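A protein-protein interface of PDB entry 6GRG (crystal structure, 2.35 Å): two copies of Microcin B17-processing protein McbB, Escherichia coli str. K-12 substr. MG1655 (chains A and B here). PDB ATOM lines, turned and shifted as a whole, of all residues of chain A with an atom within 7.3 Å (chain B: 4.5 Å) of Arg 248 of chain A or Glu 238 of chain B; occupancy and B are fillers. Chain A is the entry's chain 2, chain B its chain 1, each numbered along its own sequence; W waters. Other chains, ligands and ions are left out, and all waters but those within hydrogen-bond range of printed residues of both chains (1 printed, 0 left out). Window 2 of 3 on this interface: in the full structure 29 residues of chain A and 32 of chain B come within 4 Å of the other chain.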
ATOM      1  N   TRP A 115     -29.191   3.164   6.344  1.00  0.00           N
ATOM      2  CA  TRP A 115     -28.690   1.850   6.812  1.00  0.00           C
ATOM      3  C   TRP A 115     -29.817   0.875   7.217  1.00  0.00           C
ATOM      4  O   TRP A 115     -29.589  -0.338   7.312  1.00  0.00           O
ATOM      5  CB  TRP A 115     -27.680   2.076   7.944  1.00  0.00           C
ATOM      6  CG  TRP A 115     -26.452   2.828   7.521  1.00  0.00           C
ATOM      7  CD1 TRP A 115     -26.147   3.271   6.266  1.00  0.00           C
ATOM      8  CD2 TRP A 115     -25.329   3.164   8.348  1.00  0.00           C
ATOM      9  NE1 TRP A 115     -24.920   3.870   6.262  1.00  0.00           N
ATOM     10  CE2 TRP A 115     -24.400   3.830   7.528  1.00  0.00           C
ATOM     11  CE3 TRP A 115     -25.032   2.997   9.702  1.00  0.00           C
ATOM     12  CZ2 TRP A 115     -23.187   4.315   8.019  1.00  0.00           C
ATOM     13  CZ3 TRP A 115     -23.837   3.475  10.190  1.00  0.00           C
ATOM     14  CH2 TRP A 115     -22.922   4.116   9.354  1.00  0.00           C
ATOM     15  N   ASP A 118     -29.964  -1.939   4.923  1.00  0.00           N
ATOM     16  CA  ASP A 118     -28.946  -2.907   5.201  1.00  0.00           C
ATOM     17  C   ASP A 118     -29.330  -3.739   6.430  1.00  0.00           C
ATOM     18  O   ASP A 118     -28.557  -4.572   6.868  1.00  0.00           O
ATOM     19  CB  ASP A 118     -27.607  -2.189   5.382  1.00  0.00           C
ATOM     20  CG  ASP A 118     -27.216  -1.463   4.107  1.00  0.00           C
ATOM     21  OD1 ASP A 118     -26.934  -2.174   3.097  1.00  0.00           O
ATOM     22  OD2 ASP A 118     -27.266  -0.206   4.100  1.00  0.00           O
ATOM     23  N   VAL A 120     -29.679  -2.308   9.432  1.00  0.00           N
ATOM     24  CA  VAL A 120     -28.898  -1.725  10.532  1.00  0.00           C
ATOM     25  C   VAL A 120     -29.712  -0.588  11.158  1.00  0.00           C
ATOM     26  O   VAL A 120     -30.150   0.318  10.458  1.00  0.00           O
ATOM     27  CB  VAL A 120     -27.520  -1.223  10.074  1.00  0.00           C
ATOM     28  CG1 VAL A 120     -26.857  -0.423  11.173  1.00  0.00           C
ATOM     29  CG2 VAL A 120     -26.617  -2.348   9.605  1.00  0.00           C
ATOM     30  N   TRP A 142     -21.530   3.209  19.576  1.00  0.00           N
ATOM     31  CA  TRP A 142     -20.440   3.404  18.644  1.00  0.00           C
ATOM     32  C   TRP A 142     -19.841   4.800  18.856  1.00  0.00           C
ATOM     33  O   TRP A 142     -20.444   5.820  18.504  1.00  0.00           O
ATOM     34  CB  TRP A 142     -20.868   3.195  17.180  1.00  0.00           C
ATOM     35  CG  TRP A 142     -19.665   3.063  16.301  1.00  0.00           C
ATOM     36  CD1 TRP A 142     -18.663   3.980  16.167  1.00  0.00           C
ATOM     37  CD2 TRP A 142     -19.283   1.927  15.500  1.00  0.00           C
ATOM     38  NE1 TRP A 142     -17.708   3.513  15.299  1.00  0.00           N
ATOM     39  CE2 TRP A 142     -18.037   2.240  14.906  1.00  0.00           C
ATOM     40  CE3 TRP A 142     -19.872   0.697  15.205  1.00  0.00           C
ATOM     41  CZ2 TRP A 142     -17.360   1.357  14.057  1.00  0.00           C
ATOM     42  CZ3 TRP A 142     -19.205  -0.175  14.365  1.00  0.00           C
ATOM     43  CH2 TRP A 142     -17.963   0.147  13.805  1.00  0.00           C
ATOM     44  N   GLY A 240     -15.836   8.714   3.362  1.00  0.00           N
ATOM     45  CA  GLY A 240     -16.678   7.755   2.686  1.00  0.00           C
ATOM     46  C   GLY A 240     -16.256   6.321   2.966  1.00  0.00           C
ATOM     47  O   GLY A 240     -17.073   5.488   3.268  1.00  0.00           O
ATOM     48  N   SER A 242     -14.476   5.222   5.503  1.00  0.00           N
ATOM     49  CA  SER A 242     -14.734   5.022   6.952  1.00  0.00           C
ATOM     50  C   SER A 242     -16.201   4.665   7.203  1.00  0.00           C
ATOM     51  O   SER A 242     -16.503   3.701   7.865  1.00  0.00           O
ATOM     52  CB  SER A 242     -14.354   6.243   7.736  1.00  0.00           C
ATOM     53  OG  SER A 242     -12.946   6.392   7.760  1.00  0.00           O
ATOM     54  N   TYR A 243     -17.078   5.501   6.669  1.00  0.00           N
ATOM     55  CA  TYR A 243     -18.523   5.386   6.733  1.00  0.00           C
ATOM     56  C   TYR A 243     -18.978   3.959   6.393  1.00  0.00           C
ATOM     57  O   TYR A 243     -19.866   3.408   7.062  1.00  0.00           O
ATOM     58  CB  TYR A 243     -19.111   6.425   5.774  1.00  0.00           C
ATOM     59  CG  TYR A 243     -20.596   6.654   5.851  1.00  0.00           C
ATOM     60  CD1 TYR A 243     -21.174   7.391   6.876  1.00  0.00           C
ATOM     61  CD2 TYR A 243     -21.416   6.204   4.837  1.00  0.00           C
ATOM     62  CE1 TYR A 243     -22.541   7.644   6.894  1.00  0.00           C
ATOM     63  CE2 TYR A 243     -22.778   6.440   4.842  1.00  0.00           C
ATOM     64  CZ  TYR A 243     -23.342   7.172   5.865  1.00  0.00           C
ATOM     65  OH  TYR A 243     -24.686   7.402   5.823  1.00  0.00           O
ATOM     66  N   HIS A 244     -18.377   3.377   5.345  1.00  0.00           N
ATOM     67  CA  HIS A 244     -18.824   2.112   4.814  1.00  0.00           C
ATOM     68  C   HIS A 244     -18.340   0.998   5.748  1.00  0.00           C
ATOM     69  O   HIS A 244     -19.056   0.038   6.020  1.00  0.00           O
ATOM     70  CB  HIS A 244     -18.378   1.958   3.348  1.00  0.00           C
ATOM     71  CG  HIS A 244     -18.732   0.649   2.735  1.00  0.00           C
ATOM     72  ND1 HIS A 244     -20.040   0.253   2.532  1.00  0.00           N
ATOM     73  CD2 HIS A 244     -17.961  -0.365   2.299  1.00  0.00           C
ATOM     74  CE1 HIS A 244     -20.054  -0.939   1.983  1.00  0.00           C
ATOM     75  NE2 HIS A 244     -18.803  -1.346   1.846  1.00  0.00           N
ATOM     76  N   LEU A 245     -17.111   1.133   6.244  1.00  0.00           N
ATOM     77  CA  LEU A 245     -16.557   0.142   7.161  1.00  0.00           C
ATOM     78  C   LEU A 245     -17.450   0.103   8.396  1.00  0.00           C
ATOM     79  O   LEU A 245     -17.755  -0.968   8.872  1.00  0.00           O
ATOM     80  CB  LEU A 245     -15.107   0.488   7.518  1.00  0.00           C
ATOM     81  CG  LEU A 245     -14.072   0.269   6.414  1.00  0.00           C
ATOM     82  CD1 LEU A 245     -12.655   0.313   6.971  1.00  0.00           C
ATOM     83  CD2 LEU A 245     -14.298  -1.039   5.705  1.00  0.00           C
ATOM     84  N   ILE A 246     -17.888   1.281   8.866  1.00  0.00           N
ATOM     85  CA  ILE A 246     -18.698   1.382  10.040  1.00  0.00           C
ATOM     86  C   ILE A 246     -20.009   0.646   9.748  1.00  0.00           C
ATOM     87  O   ILE A 246     -20.421  -0.216  10.539  1.00  0.00           O
ATOM     88  CB  ILE A 246     -18.905   2.848  10.458  1.00  0.00           C
ATOM     89  CG1 ILE A 246     -17.617   3.465  10.997  1.00  0.00           C
ATOM     90  CG2 ILE A 246     -20.046   2.994  11.454  1.00  0.00           C
ATOM     91  CD1 ILE A 246     -17.642   4.979  10.974  1.00  0.00           C
ATOM     92  N   LYS A 247     -20.625   0.959   8.602  1.00  0.00           N
ATOM     93  CA  LYS A 247     -21.913   0.364   8.266  1.00  0.00           C
ATOM     94  C   LYS A 247     -21.788  -1.158   8.279  1.00  0.00           C
ATOM     95  O   LYS A 247     -22.707  -1.838   8.725  1.00  0.00           O
ATOM     96  CB  LYS A 247     -22.445   0.780   6.895  1.00  0.00           C
ATOM     97  CG  LYS A 247     -23.896   0.372   6.647  1.00  0.00           C
ATOM     98  CD  LYS A 247     -24.379   0.623   5.247  1.00  0.00           C
ATOM     99  CE  LYS A 247     -24.034  -0.543   4.346  1.00  0.00           C
ATOM    100  NZ  LYS A 247     -24.101  -0.191   2.909  1.00  0.00           N
ATOM    101  N   ARG A 248     -20.668  -1.681   7.763  1.00  0.00           N
ATOM    102  CA  ARG A 248     -20.579  -3.112   7.528  1.00  0.00           C
ATOM    103  C   ARG A 248     -20.253  -3.843   8.837  1.00  0.00           C
ATOM    104  O   ARG A 248     -20.703  -4.938   9.023  1.00  0.00           O
ATOM    105  CB  ARG A 248     -19.560  -3.427   6.430  1.00  0.00           C
ATOM    106  CG  ARG A 248     -20.084  -3.206   5.023  1.00  0.00           C
ATOM    107  CD  ARG A 248     -21.317  -4.030   4.669  1.00  0.00           C
ATOM    108  NE  ARG A 248     -21.590  -3.901   3.249  1.00  0.00           N
ATOM    109  CZ  ARG A 248     -22.773  -4.061   2.658  1.00  0.00           C
ATOM    110  NH1 ARG A 248     -23.833  -4.407   3.368  1.00  0.00           N
ATOM    111  NH2 ARG A 248     -22.878  -3.870   1.351  1.00  0.00           N
ATOM    112  N   ARG A 249     -19.477  -3.232   9.738  1.00  0.00           N
ATOM    113  CA  ARG A 249     -19.245  -3.812  11.097  1.00  0.00           C
ATOM    114  C   ARG A 249     -20.533  -3.861  11.940  1.00  0.00           C
ATOM    115  O   ARG A 249     -20.758  -4.827  12.676  1.00  0.00           O
ATOM    116  CB  ARG A 249     -18.235  -2.988  11.894  1.00  0.00           C
ATOM    117  CG  ARG A 249     -17.757  -3.695  13.154  1.00  0.00           C
ATOM    118  CD  ARG A 249     -17.034  -4.977  12.804  1.00  0.00           C
ATOM    119  NE  ARG A 249     -16.444  -5.614  13.951  1.00  0.00           N
ATOM    120  CZ  ARG A 249     -16.926  -6.690  14.564  1.00  0.00           C
ATOM    121  NH1 ARG A 249     -17.854  -7.439  13.987  1.00  0.00           N
ATOM    122  NH2 ARG A 249     -16.462  -7.015  15.763  1.00  0.00           N
ATOM    123  N   LEU A 250     -21.313  -2.772  11.905  1.00  0.00           N
ATOM    124  CA  LEU A 250     -22.618  -2.694  12.560  1.00  0.00           C
ATOM    125  C   LEU A 250     -23.560  -3.780  12.016  1.00  0.00           C
ATOM    126  O   LEU A 250     -24.259  -4.420  12.784  1.00  0.00           O
ATOM    127  CB  LEU A 250     -23.237  -1.327  12.278  1.00  0.00           C
ATOM    128  CG  LEU A 250     -22.915  -0.218  13.254  1.00  0.00           C
ATOM    129  CD1 LEU A 250     -23.485   1.089  12.734  1.00  0.00           C
ATOM    130  CD2 LEU A 250     -23.488  -0.550  14.612  1.00  0.00           C
ATOM    131  N   GLN A 251     -23.595  -3.951  10.687  1.00  0.00           N
ATOM    132  CA  GLN A 251     -24.266  -5.082  10.072  1.00  0.00           C
ATOM    133  C   GLN A 251     -23.761  -6.405  10.685  1.00  0.00           C
ATOM    134  O   GLN A 251     -24.537  -7.284  11.001  1.00  0.00           O
ATOM    135  CB  GLN A 251     -24.097  -5.032   8.556  1.00  0.00           C
ATOM    136  CG  GLN A 251     -24.924  -6.080   7.813  1.00  0.00           C
ATOM    137  CD  GLN A 251     -24.916  -5.844   6.320  1.00  0.00           C
ATOM    138  OE1 GLN A 251     -23.872  -5.871   5.665  1.00  0.00           O
ATOM    139  NE2 GLN A 251     -26.090  -5.598   5.763  1.00  0.00           N
ATOM    140  N   GLU A 252     -22.454  -6.554  10.871  1.00  0.00           N
ATOM    141  CA  GLU A 252     -21.887  -7.787  11.456  1.00  0.00           C
ATOM    142  C   GLU A 252     -22.378  -7.961  12.896  1.00  0.00           C
ATOM    143  O   GLU A 252     -22.428  -9.064  13.378  1.00  0.00           O
ATOM    144  CB  GLU A 252     -20.352  -7.773  11.514  1.00  0.00           C
ATOM    145  CG  GLU A 252     -19.653  -8.407  10.330  1.00  0.00           C
ATOM    146  CD  GLU A 252     -18.183  -8.015  10.202  1.00  0.00           C
ATOM    147  OE1 GLU A 252     -17.550  -7.735  11.245  1.00  0.00           O
ATOM    148  OE2 GLU A 252     -17.663  -7.986   9.052  1.00  0.00           O
ATOM    149  N   LEU A 253     -22.627  -6.855  13.603  1.00  0.00           N
ATOM    150  CA  LEU A 253     -22.967  -6.927  15.023  1.00  0.00           C
ATOM    151  C   LEU A 253     -24.480  -6.946  15.241  1.00  0.00           C
ATOM    152  O   LEU A 253     -24.874  -6.989  16.397  1.00  0.00           O
ATOM    153  CB  LEU A 253     -22.315  -5.752  15.748  1.00  0.00           C
ATOM    154  CG  LEU A 253     -20.789  -5.855  15.823  1.00  0.00           C
ATOM    155  CD1 LEU A 253     -20.148  -4.621  16.428  1.00  0.00           C
ATOM    156  CD2 LEU A 253     -20.369  -7.100  16.584  1.00  0.00           C
ATOM    157  N   THR A 254     -25.274  -6.951  14.151  1.00  0.00           N
ATOM    158  CA  THR A 254     -26.742  -6.935  14.153  1.00  0.00           C
ATOM    159  C   THR A 254     -27.300  -8.366  14.118  1.00  0.00           C
ATOM    160  O   THR A 254     -26.817  -9.209  13.356  1.00  0.00           O
ATOM    161  CB  THR A 254     -27.306  -6.189  12.937  1.00  0.00           C
ATOM    162  OG1 THR A 254     -26.813  -4.850  12.990  1.00  0.00           O
ATOM    163  CG2 THR A 254     -28.822  -6.180  12.898  1.00  0.00           C
ATOM    164  N   LEU B 234     -26.776  -0.116  -4.835  1.00  0.00           N
ATOM    165  CA  LEU B 234     -25.795   0.658  -4.137  1.00  0.00           C
ATOM    166  C   LEU B 234     -26.505   1.645  -3.203  1.00  0.00           C
ATOM    167  O   LEU B 234     -27.548   2.158  -3.554  1.00  0.00           O
ATOM    168  CB  LEU B 234     -24.967   1.429  -5.161  1.00  0.00           C
ATOM    169  CG  LEU B 234     -24.196   0.589  -6.167  1.00  0.00           C
ATOM    170  CD1 LEU B 234     -23.488   1.511  -7.136  1.00  0.00           C
ATOM    171  CD2 LEU B 234     -23.198  -0.325  -5.477  1.00  0.00           C
ATOM    172  N   GLY B 235     -25.919   1.886  -2.022  1.00  0.00           N
ATOM    173  CA  GLY B 235     -26.272   3.012  -1.165  1.00  0.00           C
ATOM    174  C   GLY B 235     -25.190   4.065  -1.275  1.00  0.00           C
ATOM    175  O   GLY B 235     -24.240   3.855  -2.030  1.00  0.00           O
ATOM    176  N   GLU B 236     -25.322   5.162  -0.513  1.00  0.00           N
ATOM    177  CA  GLU B 236     -24.320   6.237  -0.450  1.00  0.00           C
ATOM    178  C   GLU B 236     -22.980   5.659   0.066  1.00  0.00           C
ATOM    179  O   GLU B 236     -21.888   6.070  -0.384  1.00  0.00           O
ATOM    180  CB  GLU B 236     -24.900   7.392   0.377  1.00  0.00           C
ATOM    181  CG  GLU B 236     -24.048   8.665   0.375  1.00  0.00           C
ATOM    182  CD  GLU B 236     -24.114   9.569   1.611  1.00  0.00           C
ATOM    183  OE1 GLU B 236     -25.225   9.999   1.982  1.00  0.00           O
ATOM    184  OE2 GLU B 236     -23.045   9.838   2.214  1.00  0.00           O
ATOM    185  N   SER B 237     -23.046   4.650   0.952  1.00  0.00           N
ATOM    186  CA  SER B 237     -21.856   4.071   1.579  1.00  0.00           C
ATOM    187  C   SER B 237     -21.026   3.258   0.574  1.00  0.00           C
ATOM    188  O   SER B 237     -19.796   3.375   0.551  1.00  0.00           O
ATOM    189  CB  SER B 237     -22.199   3.268   2.809  1.00  0.00           C
ATOM    190  OG  SER B 237     -22.076   1.879   2.588  1.00  0.00           O
ATOM    191  N   GLU B 238     -21.673   2.433  -0.251  1.00  0.00           N
ATOM    192  CA  GLU B 238     -20.940   1.706  -1.316  1.00  0.00           C
ATOM    193  C   GLU B 238     -20.317   2.717  -2.282  1.00  0.00           C
ATOM    194  O   GLU B 238     -19.191   2.556  -2.706  1.00  0.00           O
ATOM    195  CB  GLU B 238     -21.850   0.732  -2.067  1.00  0.00           C
ATOM    196  CG  GLU B 238     -22.172  -0.556  -1.308  1.00  0.00           C
ATOM    197  CD  GLU B 238     -23.207  -0.406  -0.213  1.00  0.00           C
ATOM    198  OE1 GLU B 238     -23.998   0.558  -0.289  1.00  0.00           O
ATOM    199  OE2 GLU B 238     -23.200  -1.236   0.731  1.00  0.00           O
ATOM    200  N   ARG B 239     -21.049   3.782  -2.606  1.00  0.00           N
ATOM    201  CA  ARG B 239     -20.518   4.831  -3.500  1.00  0.00           C
ATOM    202  C   ARG B 239     -19.286   5.492  -2.903  1.00  0.00           C
ATOM    203  O   ARG B 239     -18.332   5.749  -3.653  1.00  0.00           O
ATOM    204  CB  ARG B 239     -21.513   5.959  -3.766  1.00  0.00           C
ATOM    205  CG  ARG B 239     -22.333   5.748  -5.025  1.00  0.00           C
ATOM    206  CD  ARG B 239     -23.743   6.225  -4.875  1.00  0.00           C
ATOM    207  NE  ARG B 239     -24.528   5.495  -5.831  1.00  0.00           N
ATOM    208  CZ  ARG B 239     -25.827   5.302  -5.756  1.00  0.00           C
ATOM    209  NH1 ARG B 239     -26.508   5.784  -4.733  1.00  0.00           N
ATOM    210  NH2 ARG B 239     -26.421   4.608  -6.713  1.00  0.00           N
ATOM    211  N   GLY B 240     -19.347   5.788  -1.588  1.00  0.00           N
ATOM    212  CA  GLY B 240     -18.241   6.384  -0.833  1.00  0.00           C
ATOM    213  C   GLY B 240     -16.982   5.544  -0.869  1.00  0.00           C
ATOM    214  O   GLY B 240     -15.895   6.040  -1.160  1.00  0.00           O
ATOM    215  N   PHE B 241     -17.142   4.265  -0.551  1.00  0.00           N
ATOM    216  CA  PHE B 241     -16.076   3.269  -0.627  1.00  0.00           C
ATOM    217  C   PHE B 241     -15.460   3.241  -2.033  1.00  0.00           C
ATOM    218  O   PHE B 241     -14.237   3.203  -2.194  1.00  0.00           O
ATOM    219  CB  PHE B 241     -16.666   1.902  -0.276  1.00  0.00           C
ATOM    220  CG  PHE B 241     -15.676   0.791  -0.074  1.00  0.00           C
ATOM    221  CD1 PHE B 241     -14.968   0.684   1.112  1.00  0.00           C
ATOM    222  CD2 PHE B 241     -15.507  -0.184  -1.036  1.00  0.00           C
ATOM    223  CE1 PHE B 241     -14.100  -0.372   1.320  1.00  0.00           C
ATOM    224  CE2 PHE B 241     -14.627  -1.232  -0.831  1.00  0.00           C
ATOM    225  CZ  PHE B 241     -13.930  -1.328   0.347  1.00  0.00           C
ATOM    226  N   SER B 242     -16.322   3.298  -3.049  1.00  0.00           N
ATOM    227  CA  SER B 242     -15.908   3.193  -4.459  1.00  0.00           C
ATOM    228  C   SER B 242     -15.065   4.416  -4.850  1.00  0.00           C
ATOM    229  O   SER B 242     -14.091   4.298  -5.585  1.00  0.00           O
ATOM    230  CB  SER B 242     -17.116   3.019  -5.388  1.00  0.00           C
ATOM    231  OG  SER B 242     -17.802   1.792  -5.149  1.00  0.00           O
ATOM    232  N   LEU B 274     -17.993  -5.693  -1.332  1.00  0.00           N
ATOM    233  CA  LEU B 274     -18.623  -4.598  -0.656  1.00  0.00           C
ATOM    234  C   LEU B 274     -19.227  -5.043   0.677  1.00  0.00           C
ATOM    235  O   LEU B 274     -19.499  -4.188   1.518  1.00  0.00           O
ATOM    236  CB  LEU B 274     -19.654  -3.985  -1.603  1.00  0.00           C
ATOM    237  CG  LEU B 274     -19.037  -3.348  -2.840  1.00  0.00           C
ATOM    238  CD1 LEU B 274     -20.075  -3.118  -3.913  1.00  0.00           C
ATOM    239  CD2 LEU B 274     -18.337  -2.052  -2.463  1.00  0.00           C
ATOM    240  N   ILE B 275     -19.390  -6.348   0.891  1.00  0.00           N
ATOM    241  CA  ILE B 275     -19.896  -6.872   2.172  1.00  0.00           C
ATOM    242  C   ILE B 275     -18.795  -6.863   3.253  1.00  0.00           C
ATOM    243  O   ILE B 275     -18.986  -6.411   4.377  1.00  0.00           O
ATOM    244  CB  ILE B 275     -20.481  -8.287   2.005  1.00  0.00           C
ATOM    245  CG1 ILE B 275     -21.458  -8.376   0.830  1.00  0.00           C
ATOM    246  CG2 ILE B 275     -21.111  -8.753   3.323  1.00  0.00           C
ATOM    247  CD1 ILE B 275     -22.538  -7.317   0.823  1.00  0.00           C
ATOM    248  N   CYS B 277     -15.480  -5.829   2.600  1.00  0.00           N
ATOM    249  CA  CYS B 277     -14.513  -4.731   2.366  1.00  0.00           C
ATOM    250  C   CYS B 277     -13.082  -5.229   2.071  1.00  0.00           C
ATOM    251  O   CYS B 277     -12.169  -4.434   2.013  1.00  0.00           O
ATOM    252  CB  CYS B 277     -14.529  -3.735   3.514  1.00  0.00           C
ATOM    253  SG  CYS B 277     -16.180  -3.052   3.787  1.00  0.00           S
HETATM  254  O   HOH W   1     -25.339   4.277   3.021  1.00  0.00           O
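The side-chain hydroxyl (OG) of Ser 237 of chain B sits at hydrogen-bond distance from a ring nitrogen (ND1) of His 244 of chain A (2.6 Å).
The side-chain amino group of Lys 247 of chain A lies within hydrogen-bond range of the side-chain hydroxyl of Ser 237 of chain B (2.9 Å).
NZ of Lys 247 of chain A is in salt-bridge range of OE2 of Glu 238 of chain B.
The side-chain carboxylate (OE2) of Glu 238 of chain B lies within salt-bridge range of the guanidinium group (NH2) of Arg 248 of chain A (2.7 Å).
The backbone carbonyl oxygen (O) of Leu 274 of chain B lies within hydrogen-bond range of a ring nitrogen (NE2) of His 244 of chain A, 2.9 Å away.
O of Leu 274 of chain B is in hydrogen-bond range of NE of Arg 248 of chain A (2.7 Å).
NE2 of His 244 of chain A lies close to SG of Cys 277 of chain B (3.7 Å).
OE1 of Glu 238 of chain B is in hydrogen-bond range of N of Gly 235 of chain B (2.9 Å).
O of Glu 238 of chain B lies within hydrogen-bond range of OG of Ser 242 of chain B, 2.9 Å away.
NZ of Lys 247 of chain A is in salt-bridge range of OD2 of Asp 118 of chain A, 3.4 Å away.
NH1 of Arg 248 of chain A is in salt-bridge range of OD1 of Asp 118 of chain A (3.8 Å).
The side-chain amide oxygen (OE1) of Gln 251 of chain A sits at hydrogen-bond distance from the guanidinium group (NH1) of Arg 248 of chain A (2.7 Å).
Among the printed residues, merely in contact across the chains: Arg 248 of chain A with Ile 275 of chain B (3.3 Å), Leu 245 of chain A with Cys 277 of chain B (3.4 Å), His 244 of chain A with Phe 241 of chain B (3.4 Å), His 244 of chain A with Glu 238 of chain B (3.4 Å), Tyr 243 of chain A with Ser 237 of chain B (3.7 Å) and Gly 240 of chain A with Gly 240 of chain B (3.98 Å).
Of the printed residues of chain B, Gly 240 of chain A touches Gly 240 (3.98 Å).
Arg 248 of chain A touches three residues of chain B.
Gln 251 of chain A touches none of the printed residues of chain B.
Ser 237 of chain B touches just these residues of chain A: Tyr 243, His 244 and Lys 247.
Glu 238 of chain B touches just these residues of chain A: His 244 (3.4 Å), Lys 247 (2.6 Å) and Arg 248 (2.7 Å).
Of the printed residues of chain A, Leu 274 of chain B touches His 244 (2.9 Å) and Arg 248 (2.7 Å).
Of the printed residues of chain A, Ile 275 of chain B touches Arg 248.
The nearest residue of chain B that does not touch Arg 248 of chain A is Cys 277 of chain B (4.1 Å).
Hydrophobic or aromatic side chains of chain B within 4 Å of the printed part of chain A: Phe 241 and Ile 275.
Along chain B the printed residues that touch a printed residue of chain A span positions 237 to 277.
Printed residues of chain A that touch a printed residue of chain B: Gly 240, Tyr 243, His 244, Leu 245, Lys 247 and Arg 248.
Hydrophobic or aromatic side chains of chain A that line the printed part of chain B: Tyr 243, His 244 and Leu 245.
Among the printed residues, 13 pairs touch across the chains.
Among the printed residues, Asp or Glu carboxylates within 4 Å of a Lys or Arg side-chain nitrogen of the other chain: Lys 247 of chain A with Glu 238 of chain B (2.6 Å) and Arg 248 of chain A with Glu 238 of chain B (2.7 Å).
Gly 240 of chain B touches its own counterpart, Gly 240 of chain A.
Of the 13 pairs that touch across the chains among the printed residues, 1 has its exchanged pair printed and touching as well.
Water W1 bridges the backbone NH of Ser 237 of chain B (3.1 Å) and the indole nitrogen of Trp 115 of chain A (3.3 Å).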
